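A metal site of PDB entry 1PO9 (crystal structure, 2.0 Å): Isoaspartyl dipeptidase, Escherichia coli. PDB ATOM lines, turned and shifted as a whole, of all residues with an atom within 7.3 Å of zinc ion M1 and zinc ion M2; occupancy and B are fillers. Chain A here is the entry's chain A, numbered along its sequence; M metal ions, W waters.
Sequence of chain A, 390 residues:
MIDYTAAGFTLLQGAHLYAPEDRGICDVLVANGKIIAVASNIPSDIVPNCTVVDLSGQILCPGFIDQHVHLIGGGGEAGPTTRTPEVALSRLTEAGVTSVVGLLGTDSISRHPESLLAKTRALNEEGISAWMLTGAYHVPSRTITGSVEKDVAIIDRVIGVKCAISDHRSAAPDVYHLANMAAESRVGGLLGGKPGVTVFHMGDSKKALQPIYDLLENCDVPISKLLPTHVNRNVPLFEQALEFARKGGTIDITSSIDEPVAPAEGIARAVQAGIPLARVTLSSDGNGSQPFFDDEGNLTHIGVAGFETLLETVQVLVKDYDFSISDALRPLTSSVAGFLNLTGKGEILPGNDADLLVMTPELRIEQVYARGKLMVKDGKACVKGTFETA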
ATOM      1  N   HIS A  68      13.178 -25.028  33.936  1.00  0.00           N
ATOM      2  CA  HIS A  68      14.079 -24.276  33.067  1.00  0.00           C
ATOM      3  C   HIS A  68      15.420 -24.989  32.978  1.00  0.00           C
ATOM      4  O   HIS A  68      16.376 -24.644  33.678  1.00  0.00           O
ATOM      5  CB  HIS A  68      14.284 -22.859  33.600  1.00  0.00           C
ATOM      6  CG  HIS A  68      14.802 -21.890  32.583  1.00  0.00           C
ATOM      7  ND1 HIS A  68      14.072 -20.813  32.143  1.00  0.00           N
ATOM      8  CD2 HIS A  68      15.983 -21.847  31.912  1.00  0.00           C
ATOM      9  CE1 HIS A  68      14.773 -20.144  31.248  1.00  0.00           C
ATOM     10  NE2 HIS A  68      15.941 -20.751  31.087  1.00  0.00           N
ATOM     11  N   VAL A  69      15.489 -25.983  32.101  1.00  0.00           N
ATOM     12  CA  VAL A  69      16.701 -26.771  31.918  1.00  0.00           C
ATOM     13  C   VAL A  69      17.033 -26.958  30.453  1.00  0.00           C
ATOM     14  O   VAL A  69      16.162 -27.293  29.650  1.00  0.00           O
ATOM     15  CB  VAL A  69      16.544 -28.170  32.571  1.00  0.00           C
ATOM     16  CG1 VAL A  69      17.831 -28.977  32.384  1.00  0.00           C
ATOM     17  CG2 VAL A  69      16.197 -28.015  34.043  1.00  0.00           C
ATOM     18  N   HIS A  70      18.296 -26.750  30.102  1.00  0.00           N
ATOM     19  CA  HIS A  70      18.756 -26.930  28.726  1.00  0.00           C
ATOM     20  C   HIS A  70      19.152 -28.396  28.604  1.00  0.00           C
ATOM     21  O   HIS A  70      20.329 -28.757  28.587  1.00  0.00           O
ATOM     22  CB  HIS A  70      19.941 -26.010  28.450  1.00  0.00           C
ATOM     23  CG  HIS A  70      19.584 -24.561  28.517  1.00  0.00           C
ATOM     24  ND1 HIS A  70      19.150 -23.844  27.424  1.00  0.00           N
ATOM     25  CD2 HIS A  70      19.515 -23.712  29.573  1.00  0.00           C
ATOM     26  CE1 HIS A  70      18.825 -22.625  27.796  1.00  0.00           C
ATOM     27  NE2 HIS A  70      19.043 -22.515  29.099  1.00  0.00           N
ATOM     28  N   LEU A 103      14.205 -26.653  27.431  1.00  0.00           N
ATOM     29  CA  LEU A 103      14.025 -25.514  26.549  1.00  0.00           C
ATOM     30  C   LEU A 103      15.335 -25.149  25.880  1.00  0.00           C
ATOM     31  O   LEU A 103      16.397 -25.654  26.254  1.00  0.00           O
ATOM     32  CB  LEU A 103      13.482 -24.320  27.354  1.00  0.00           C
ATOM     33  CG  LEU A 103      14.111 -24.066  28.734  1.00  0.00           C
ATOM     34  CD1 LEU A 103      15.585 -23.721  28.596  1.00  0.00           C
ATOM     35  CD2 LEU A 103      13.368 -22.918  29.412  1.00  0.00           C
ATOM     36  N   LEU A 104      15.247 -24.289  24.863  1.00  0.00           N
ATOM     37  CA  LEU A 104      16.433 -23.841  24.135  1.00  0.00           C
ATOM     38  C   LEU A 104      16.706 -22.403  24.540  1.00  0.00           C
ATOM     39  O   LEU A 104      15.849 -21.725  25.094  1.00  0.00           O
ATOM     40  CB  LEU A 104      16.188 -23.888  22.624  1.00  0.00           C
ATOM     41  CG  LEU A 104      15.842 -25.254  22.039  1.00  0.00           C
ATOM     42  CD1 LEU A 104      15.689 -25.146  20.519  1.00  0.00           C
ATOM     43  CD2 LEU A 104      16.930 -26.248  22.402  1.00  0.00           C
ATOM     44  N   GLY A 105      17.917 -21.935  24.233  1.00  0.00           N
ATOM     45  CA  GLY A 105      18.274 -20.588  24.600  1.00  0.00           C
ATOM     46  C   GLY A 105      18.690 -19.690  23.453  1.00  0.00           C
ATOM     47  O   GLY A 105      18.003 -19.579  22.429  1.00  0.00           O
ATOM     48  N   THR A 106      19.827 -19.030  23.641  1.00  0.00           N
ATOM     49  CA  THR A 106      20.348 -18.112  22.651  1.00  0.00           C
ATOM     50  C   THR A 106      20.540 -18.791  21.301  1.00  0.00           C
ATOM     51  O   THR A 106      20.190 -18.241  20.256  1.00  0.00           O
ATOM     52  CB  THR A 106      21.704 -17.539  23.091  1.00  0.00           C
ATOM     53  OG1 THR A 106      21.571 -16.981  24.404  1.00  0.00           O
ATOM     54  CG2 THR A 106      22.166 -16.473  22.130  1.00  0.00           C
ATOM     55  N   TYR A 137      15.162 -18.261  22.188  1.00  0.00           N
ATOM     56  CA  TYR A 137      15.253 -16.815  22.347  1.00  0.00           C
ATOM     57  C   TYR A 137      14.632 -16.141  21.128  1.00  0.00           C
ATOM     58  O   TYR A 137      13.824 -15.209  21.248  1.00  0.00           O
ATOM     59  CB  TYR A 137      16.707 -16.336  22.431  1.00  0.00           C
ATOM     60  CG  TYR A 137      17.368 -16.387  23.792  1.00  0.00           C
ATOM     61  CD1 TYR A 137      18.458 -15.563  24.066  1.00  0.00           C
ATOM     62  CD2 TYR A 137      16.952 -17.288  24.771  1.00  0.00           C
ATOM     63  CE1 TYR A 137      19.131 -15.642  25.284  1.00  0.00           C
ATOM     64  CE2 TYR A 137      17.618 -17.364  26.000  1.00  0.00           C
ATOM     65  CZ  TYR A 137      18.708 -16.542  26.240  1.00  0.00           C
ATOM     66  OH  TYR A 137      19.398 -16.628  27.436  1.00  0.00           O
ATOM     67  N   KCX A 162       8.949 -20.528  24.461  1.00  0.00           N
ATOM     68  CA  KCX A 162       9.925 -19.677  25.120  1.00  0.00           C
ATOM     69  CB  KCX A 162      11.101 -20.535  25.619  1.00  0.00           C
ATOM     70  CG  KCX A 162      12.491 -20.165  25.084  1.00  0.00           C
ATOM     71  CD  KCX A 162      13.082 -18.943  25.769  1.00  0.00           C
ATOM     72  CE  KCX A 162      13.608 -19.221  27.185  1.00  0.00           C
ATOM     73  NZ  KCX A 162      14.941 -19.819  27.216  1.00  0.00           N
ATOM     74  C   KCX A 162      10.389 -18.620  24.137  1.00  0.00           C
ATOM     75  O   KCX A 162      10.255 -18.783  22.925  1.00  0.00           O
ATOM     76  CX  KCX A 162      15.907 -19.417  28.040  1.00  0.00           C
ATOM     77  OQ1 KCX A 162      15.718 -18.477  28.850  1.00  0.00           O
ATOM     78  OQ2 KCX A 162      17.041 -19.965  28.041  1.00  0.00           O
ATOM     79  N   CYS A 163      10.905 -17.525  24.673  1.00  0.00           N
ATOM     80  CA  CYS A 163      11.419 -16.429  23.856  1.00  0.00           C
ATOM     81  C   CYS A 163      12.290 -15.593  24.774  1.00  0.00           C
ATOM     82  O   CYS A 163      12.423 -15.889  25.955  1.00  0.00           O
ATOM     83  CB  CYS A 163      10.265 -15.574  23.328  1.00  0.00           C
ATOM     84  SG  CYS A 163       9.448 -14.591  24.620  1.00  0.00           S
ATOM     85  N   ALA A 164      12.894 -14.548  24.222  1.00  0.00           N
ATOM     86  CA  ALA A 164      13.746 -13.656  24.986  1.00  0.00           C
ATOM     87  C   ALA A 164      13.362 -12.214  24.688  1.00  0.00           C
ATOM     88  O   ALA A 164      13.081 -11.867  23.530  1.00  0.00           O
ATOM     89  CB  ALA A 164      15.207 -13.888  24.639  1.00  0.00           C
ATOM     90  N   ASP A 167      16.834  -8.210  26.185  1.00  0.00           N
ATOM     91  CA  ASP A 167      18.147  -8.855  26.306  1.00  0.00           C
ATOM     92  C   ASP A 167      18.955  -8.614  25.038  1.00  0.00           C
ATOM     93  O   ASP A 167      18.419  -8.679  23.924  1.00  0.00           O
ATOM     94  CB  ASP A 167      17.953 -10.360  26.521  1.00  0.00           C
ATOM     95  CG  ASP A 167      19.268 -11.087  26.775  1.00  0.00           C
ATOM     96  OD1 ASP A 167      19.626 -11.279  27.956  1.00  0.00           O
ATOM     97  OD2 ASP A 167      19.939 -11.483  25.798  1.00  0.00           O
ATOM     98  N   ARG A 169      20.641 -10.364  23.361  1.00  0.00           N
ATOM     99  CA  ARG A 169      20.699 -11.520  22.471  1.00  0.00           C
ATOM    100  C   ARG A 169      19.306 -11.840  21.937  1.00  0.00           C
ATOM    101  O   ARG A 169      19.073 -12.940  21.422  1.00  0.00           O
ATOM    102  CB  ARG A 169      21.202 -12.755  23.208  1.00  0.00           C
ATOM    103  CG  ARG A 169      22.438 -12.548  24.049  1.00  0.00           C
ATOM    104  CD  ARG A 169      22.431 -13.620  25.109  1.00  0.00           C
ATOM    105  NE  ARG A 169      23.325 -13.325  26.217  1.00  0.00           N
ATOM    106  CZ  ARG A 169      23.214 -13.873  27.418  1.00  0.00           C
ATOM    107  NH1 ARG A 169      22.243 -14.748  27.652  1.00  0.00           N
ATOM    108  NH2 ARG A 169      24.074 -13.553  28.379  1.00  0.00           N
ATOM    109  N   PHE A 200       9.361 -15.995  29.268  1.00  0.00           N
ATOM    110  CA  PHE A 200      10.196 -14.911  28.768  1.00  0.00           C
ATOM    111  C   PHE A 200      11.569 -14.816  29.427  1.00  0.00           C
ATOM    112  O   PHE A 200      11.669 -14.478  30.615  1.00  0.00           O
ATOM    113  CB  PHE A 200       9.497 -13.555  28.969  1.00  0.00           C
ATOM    114  CG  PHE A 200       8.157 -13.460  28.320  1.00  0.00           C
ATOM    115  CD1 PHE A 200       7.042 -14.046  28.908  1.00  0.00           C
ATOM    116  CD2 PHE A 200       8.006 -12.755  27.127  1.00  0.00           C
ATOM    117  CE1 PHE A 200       5.779 -13.935  28.317  1.00  0.00           C
ATOM    118  CE2 PHE A 200       6.747 -12.631  26.535  1.00  0.00           C
ATOM    119  CZ  PHE A 200       5.640 -13.220  27.129  1.00  0.00           C
ATOM    120  N   HIS A 201      12.621 -15.102  28.668  1.00  0.00           N
ATOM    121  CA  HIS A 201      13.975 -14.978  29.198  1.00  0.00           C
ATOM    122  C   HIS A 201      14.162 -13.471  29.308  1.00  0.00           C
ATOM    123  O   HIS A 201      14.061 -12.762  28.319  1.00  0.00           O
ATOM    124  CB  HIS A 201      15.014 -15.521  28.214  1.00  0.00           C
ATOM    125  CG  HIS A 201      16.407 -15.025  28.481  1.00  0.00           C
ATOM    126  ND1 HIS A 201      17.237 -15.594  29.424  1.00  0.00           N
ATOM    127  CD2 HIS A 201      17.087 -13.964  27.986  1.00  0.00           C
ATOM    128  CE1 HIS A 201      18.369 -14.909  29.494  1.00  0.00           C
ATOM    129  NE2 HIS A 201      18.304 -13.913  28.630  1.00  0.00           N
ATOM    130  N   MET A 202      14.421 -12.999  30.522  1.00  0.00           N
ATOM    131  CA  MET A 202      14.623 -11.565  30.736  1.00  0.00           C
ATOM    132  C   MET A 202      16.105 -11.223  30.702  1.00  0.00           C
ATOM    133  O   MET A 202      16.942 -11.974  31.189  1.00  0.00           O
ATOM    134  CB  MET A 202      14.068 -11.130  32.093  1.00  0.00           C
ATOM    135  CG  MET A 202      12.573 -11.366  32.298  1.00  0.00           C
ATOM    136  SD  MET A 202      11.532 -10.790  30.947  1.00  0.00           S
ATOM    137  CE  MET A 202      11.965  -9.038  30.933  1.00  0.00           C
ATOM    138  N   THR A 229      11.258 -14.965  33.474  1.00  0.00           N
ATOM    139  CA  THR A 229      12.229 -15.735  34.248  1.00  0.00           C
ATOM    140  C   THR A 229      13.543 -14.989  34.374  1.00  0.00           C
ATOM    141  O   THR A 229      13.777 -14.008  33.671  1.00  0.00           O
ATOM    142  CB  THR A 229      12.433 -17.145  33.644  1.00  0.00           C
ATOM    143  OG1 THR A 229      13.295 -17.910  34.509  1.00  0.00           O
ATOM    144  CG2 THR A 229      13.045 -17.077  32.264  1.00  0.00           C
ATOM    145  N   HIS A 230      14.406 -15.437  35.286  1.00  0.00           N
ATOM    146  CA  HIS A 230      15.679 -14.773  35.533  1.00  0.00           C
ATOM    147  C   HIS A 230      15.385 -13.380  36.096  1.00  0.00           C
ATOM    148  O   HIS A 230      16.198 -12.474  35.973  1.00  0.00           O
ATOM    149  CB  HIS A 230      16.492 -14.625  34.242  1.00  0.00           C
ATOM    150  CG  HIS A 230      16.752 -15.920  33.527  1.00  0.00           C
ATOM    151  ND1 HIS A 230      17.305 -17.015  34.151  1.00  0.00           N
ATOM    152  CD2 HIS A 230      16.528 -16.281  32.242  1.00  0.00           C
ATOM    153  CE1 HIS A 230      17.410 -18.006  33.279  1.00  0.00           C
ATOM    154  NE2 HIS A 230      16.942 -17.588  32.120  1.00  0.00           N
ATOM    155  N   ARG A 233      18.044 -11.278  38.019  1.00  0.00           N
ATOM    156  CA  ARG A 233      19.306 -10.888  37.371  1.00  0.00           C
ATOM    157  C   ARG A 233      19.721  -9.440  37.633  1.00  0.00           C
ATOM    158  O   ARG A 233      20.911  -9.115  37.550  1.00  0.00           O
ATOM    159  CB  ARG A 233      19.245 -11.132  35.871  1.00  0.00           C
ATOM    160  CG  ARG A 233      18.197 -10.301  35.168  1.00  0.00           C
ATOM    161  CD  ARG A 233      18.495 -10.179  33.675  1.00  0.00           C
ATOM    162  NE  ARG A 233      18.662 -11.475  33.028  1.00  0.00           N
ATOM    163  CZ  ARG A 233      19.830 -11.978  32.640  1.00  0.00           C
ATOM    164  NH1 ARG A 233      20.947 -11.289  32.814  1.00  0.00           N
ATOM    165  NH2 ARG A 233      19.881 -13.163  32.064  1.00  0.00           N
ATOM    166  N   THR A 254      15.648 -17.532  39.207  1.00  0.00           N
ATOM    167  CA  THR A 254      16.655 -18.519  38.816  1.00  0.00           C
ATOM    168  C   THR A 254      17.642 -18.792  39.948  1.00  0.00           C
ATOM    169  O   THR A 254      18.273 -17.879  40.470  1.00  0.00           O
ATOM    170  CB  THR A 254      17.421 -18.068  37.561  1.00  0.00           C
ATOM    171  OG1 THR A 254      16.485 -17.800  36.511  1.00  0.00           O
ATOM    172  CG2 THR A 254      18.370 -19.166  37.119  1.00  0.00           C
ATOM    173  N   SER A 284      16.466 -23.816  37.702  1.00  0.00           N
ATOM    174  CA  SER A 284      17.925 -23.791  37.731  1.00  0.00           C
ATOM    175  C   SER A 284      18.662 -23.231  36.520  1.00  0.00           C
ATOM    176  O   SER A 284      19.781 -22.732  36.655  1.00  0.00           O
ATOM    177  CB  SER A 284      18.443 -25.215  37.966  1.00  0.00           C
ATOM    178  OG  SER A 284      18.147 -26.041  36.851  1.00  0.00           O
ATOM    179  N   ASP A 285      18.038 -23.330  35.355  1.00  0.00           N
ATOM    180  CA  ASP A 285      18.667 -22.914  34.112  1.00  0.00           C
ATOM    181  C   ASP A 285      19.875 -23.824  33.990  1.00  0.00           C
ATOM    182  O   ASP A 285      20.949 -23.431  33.548  1.00  0.00           O
ATOM    183  CB  ASP A 285      19.107 -21.444  34.170  1.00  0.00           C
ATOM    184  CG  ASP A 285      19.457 -20.898  32.799  1.00  0.00           C
ATOM    185  OD1 ASP A 285      18.979 -21.469  31.791  1.00  0.00           O
ATOM    186  OD2 ASP A 285      20.199 -19.890  32.720  1.00  0.00           O
ATOM    187  N   GLY A 286      19.665 -25.071  34.418  1.00  0.00           N
ATOM    188  CA  GLY A 286      20.710 -26.068  34.404  1.00  0.00           C
ATOM    189  C   GLY A 286      21.271 -26.357  33.025  1.00  0.00           C
ATOM    190  O   GLY A 286      20.528 -26.396  32.034  1.00  0.00           O
ATOM    191  N   GLY A 288      22.951 -24.535  31.274  1.00  0.00           N
ATOM    192  CA  GLY A 288      22.941 -23.347  30.425  1.00  0.00           C
ATOM    193  C   GLY A 288      24.271 -22.610  30.494  1.00  0.00           C
ATOM    194  O   GLY A 288      25.301 -23.205  30.828  1.00  0.00           O
HETATM  195 ZN    ZN M   1      17.927 -20.732  29.884  1.00  0.00          ZN
HETATM  196 ZN    ZN M   2      17.370 -17.503  29.839  1.00  0.00          ZN
HETATM  197  O   HOH W   1      18.805 -18.934  30.116  1.00  0.00           O
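O of Cys 163 lies within hydrogen-bond range of N of His 201.
A ring nitrogen (NE2) of His 201 sits at hydrogen-bond distance from the side-chain carboxylate (OD1) of Asp 167.
The backbone carbonyl oxygen of Leu 104 lies within hydrogen-bond range of NZ of KCX 162 (3.0 Å).
ND1 of His 70 sits at hydrogen-bond distance from O of Leu 103, at 3.5 Å.
N of His 70 lies within hydrogen-bond range of O of Gly 286, 3.0 Å away.
The side-chain hydroxyl (OG1) of Thr 254 is in hydrogen-bond range of a ring nitrogen (ND1) of His 230 (2.6 Å).
OH of Tyr 137 lies within hydrogen-bond range of NH1 of Arg 169 (3.4 Å).
The backbone carbonyl oxygen (O) of Tyr 137 lies within hydrogen-bond range of the backbone NH (N) of Ala 164, at 3.2 Å.
Within 4 Å of zinc ion M1: His 68, His 70, KCX 162, His 230 and Asp 285.
The nearest printed residue that does not touch zinc ion M1 is Leu 103 (4.01 Å).
Merely in contact with zinc ion M2: Tyr 137.
The nearest printed residue that does not touch zinc ion M2 is Asp 285 (4.7 Å).
Zinc ion M1 is bound by water W1 (2.0 Å).
OQ2 of KCX 162 is bound to zinc ion M1 (2.2 Å).
NE2 of His 70 is bound to zinc ion M1 (2.2 Å).
OD1 of Asp 285 is bound to zinc ion M1, 2.3 Å away.
NE2 of His 68 is bound to zinc ion M1, 2.3 Å away.
Zinc ion M1 has five donor atoms within binding distance.
Zinc ion M2 is bound by a ring nitrogen (ND1) of His 201 (2.0 Å).
Water W1 binds zinc ion M2, 2.0 Å away.
OQ1 of KCX 162 binds zinc ion M2, at 2.2 Å.
Zinc ion M2 is bound by NE2 of His 230.
Zinc ion M2 has four donor atoms within binding distance.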
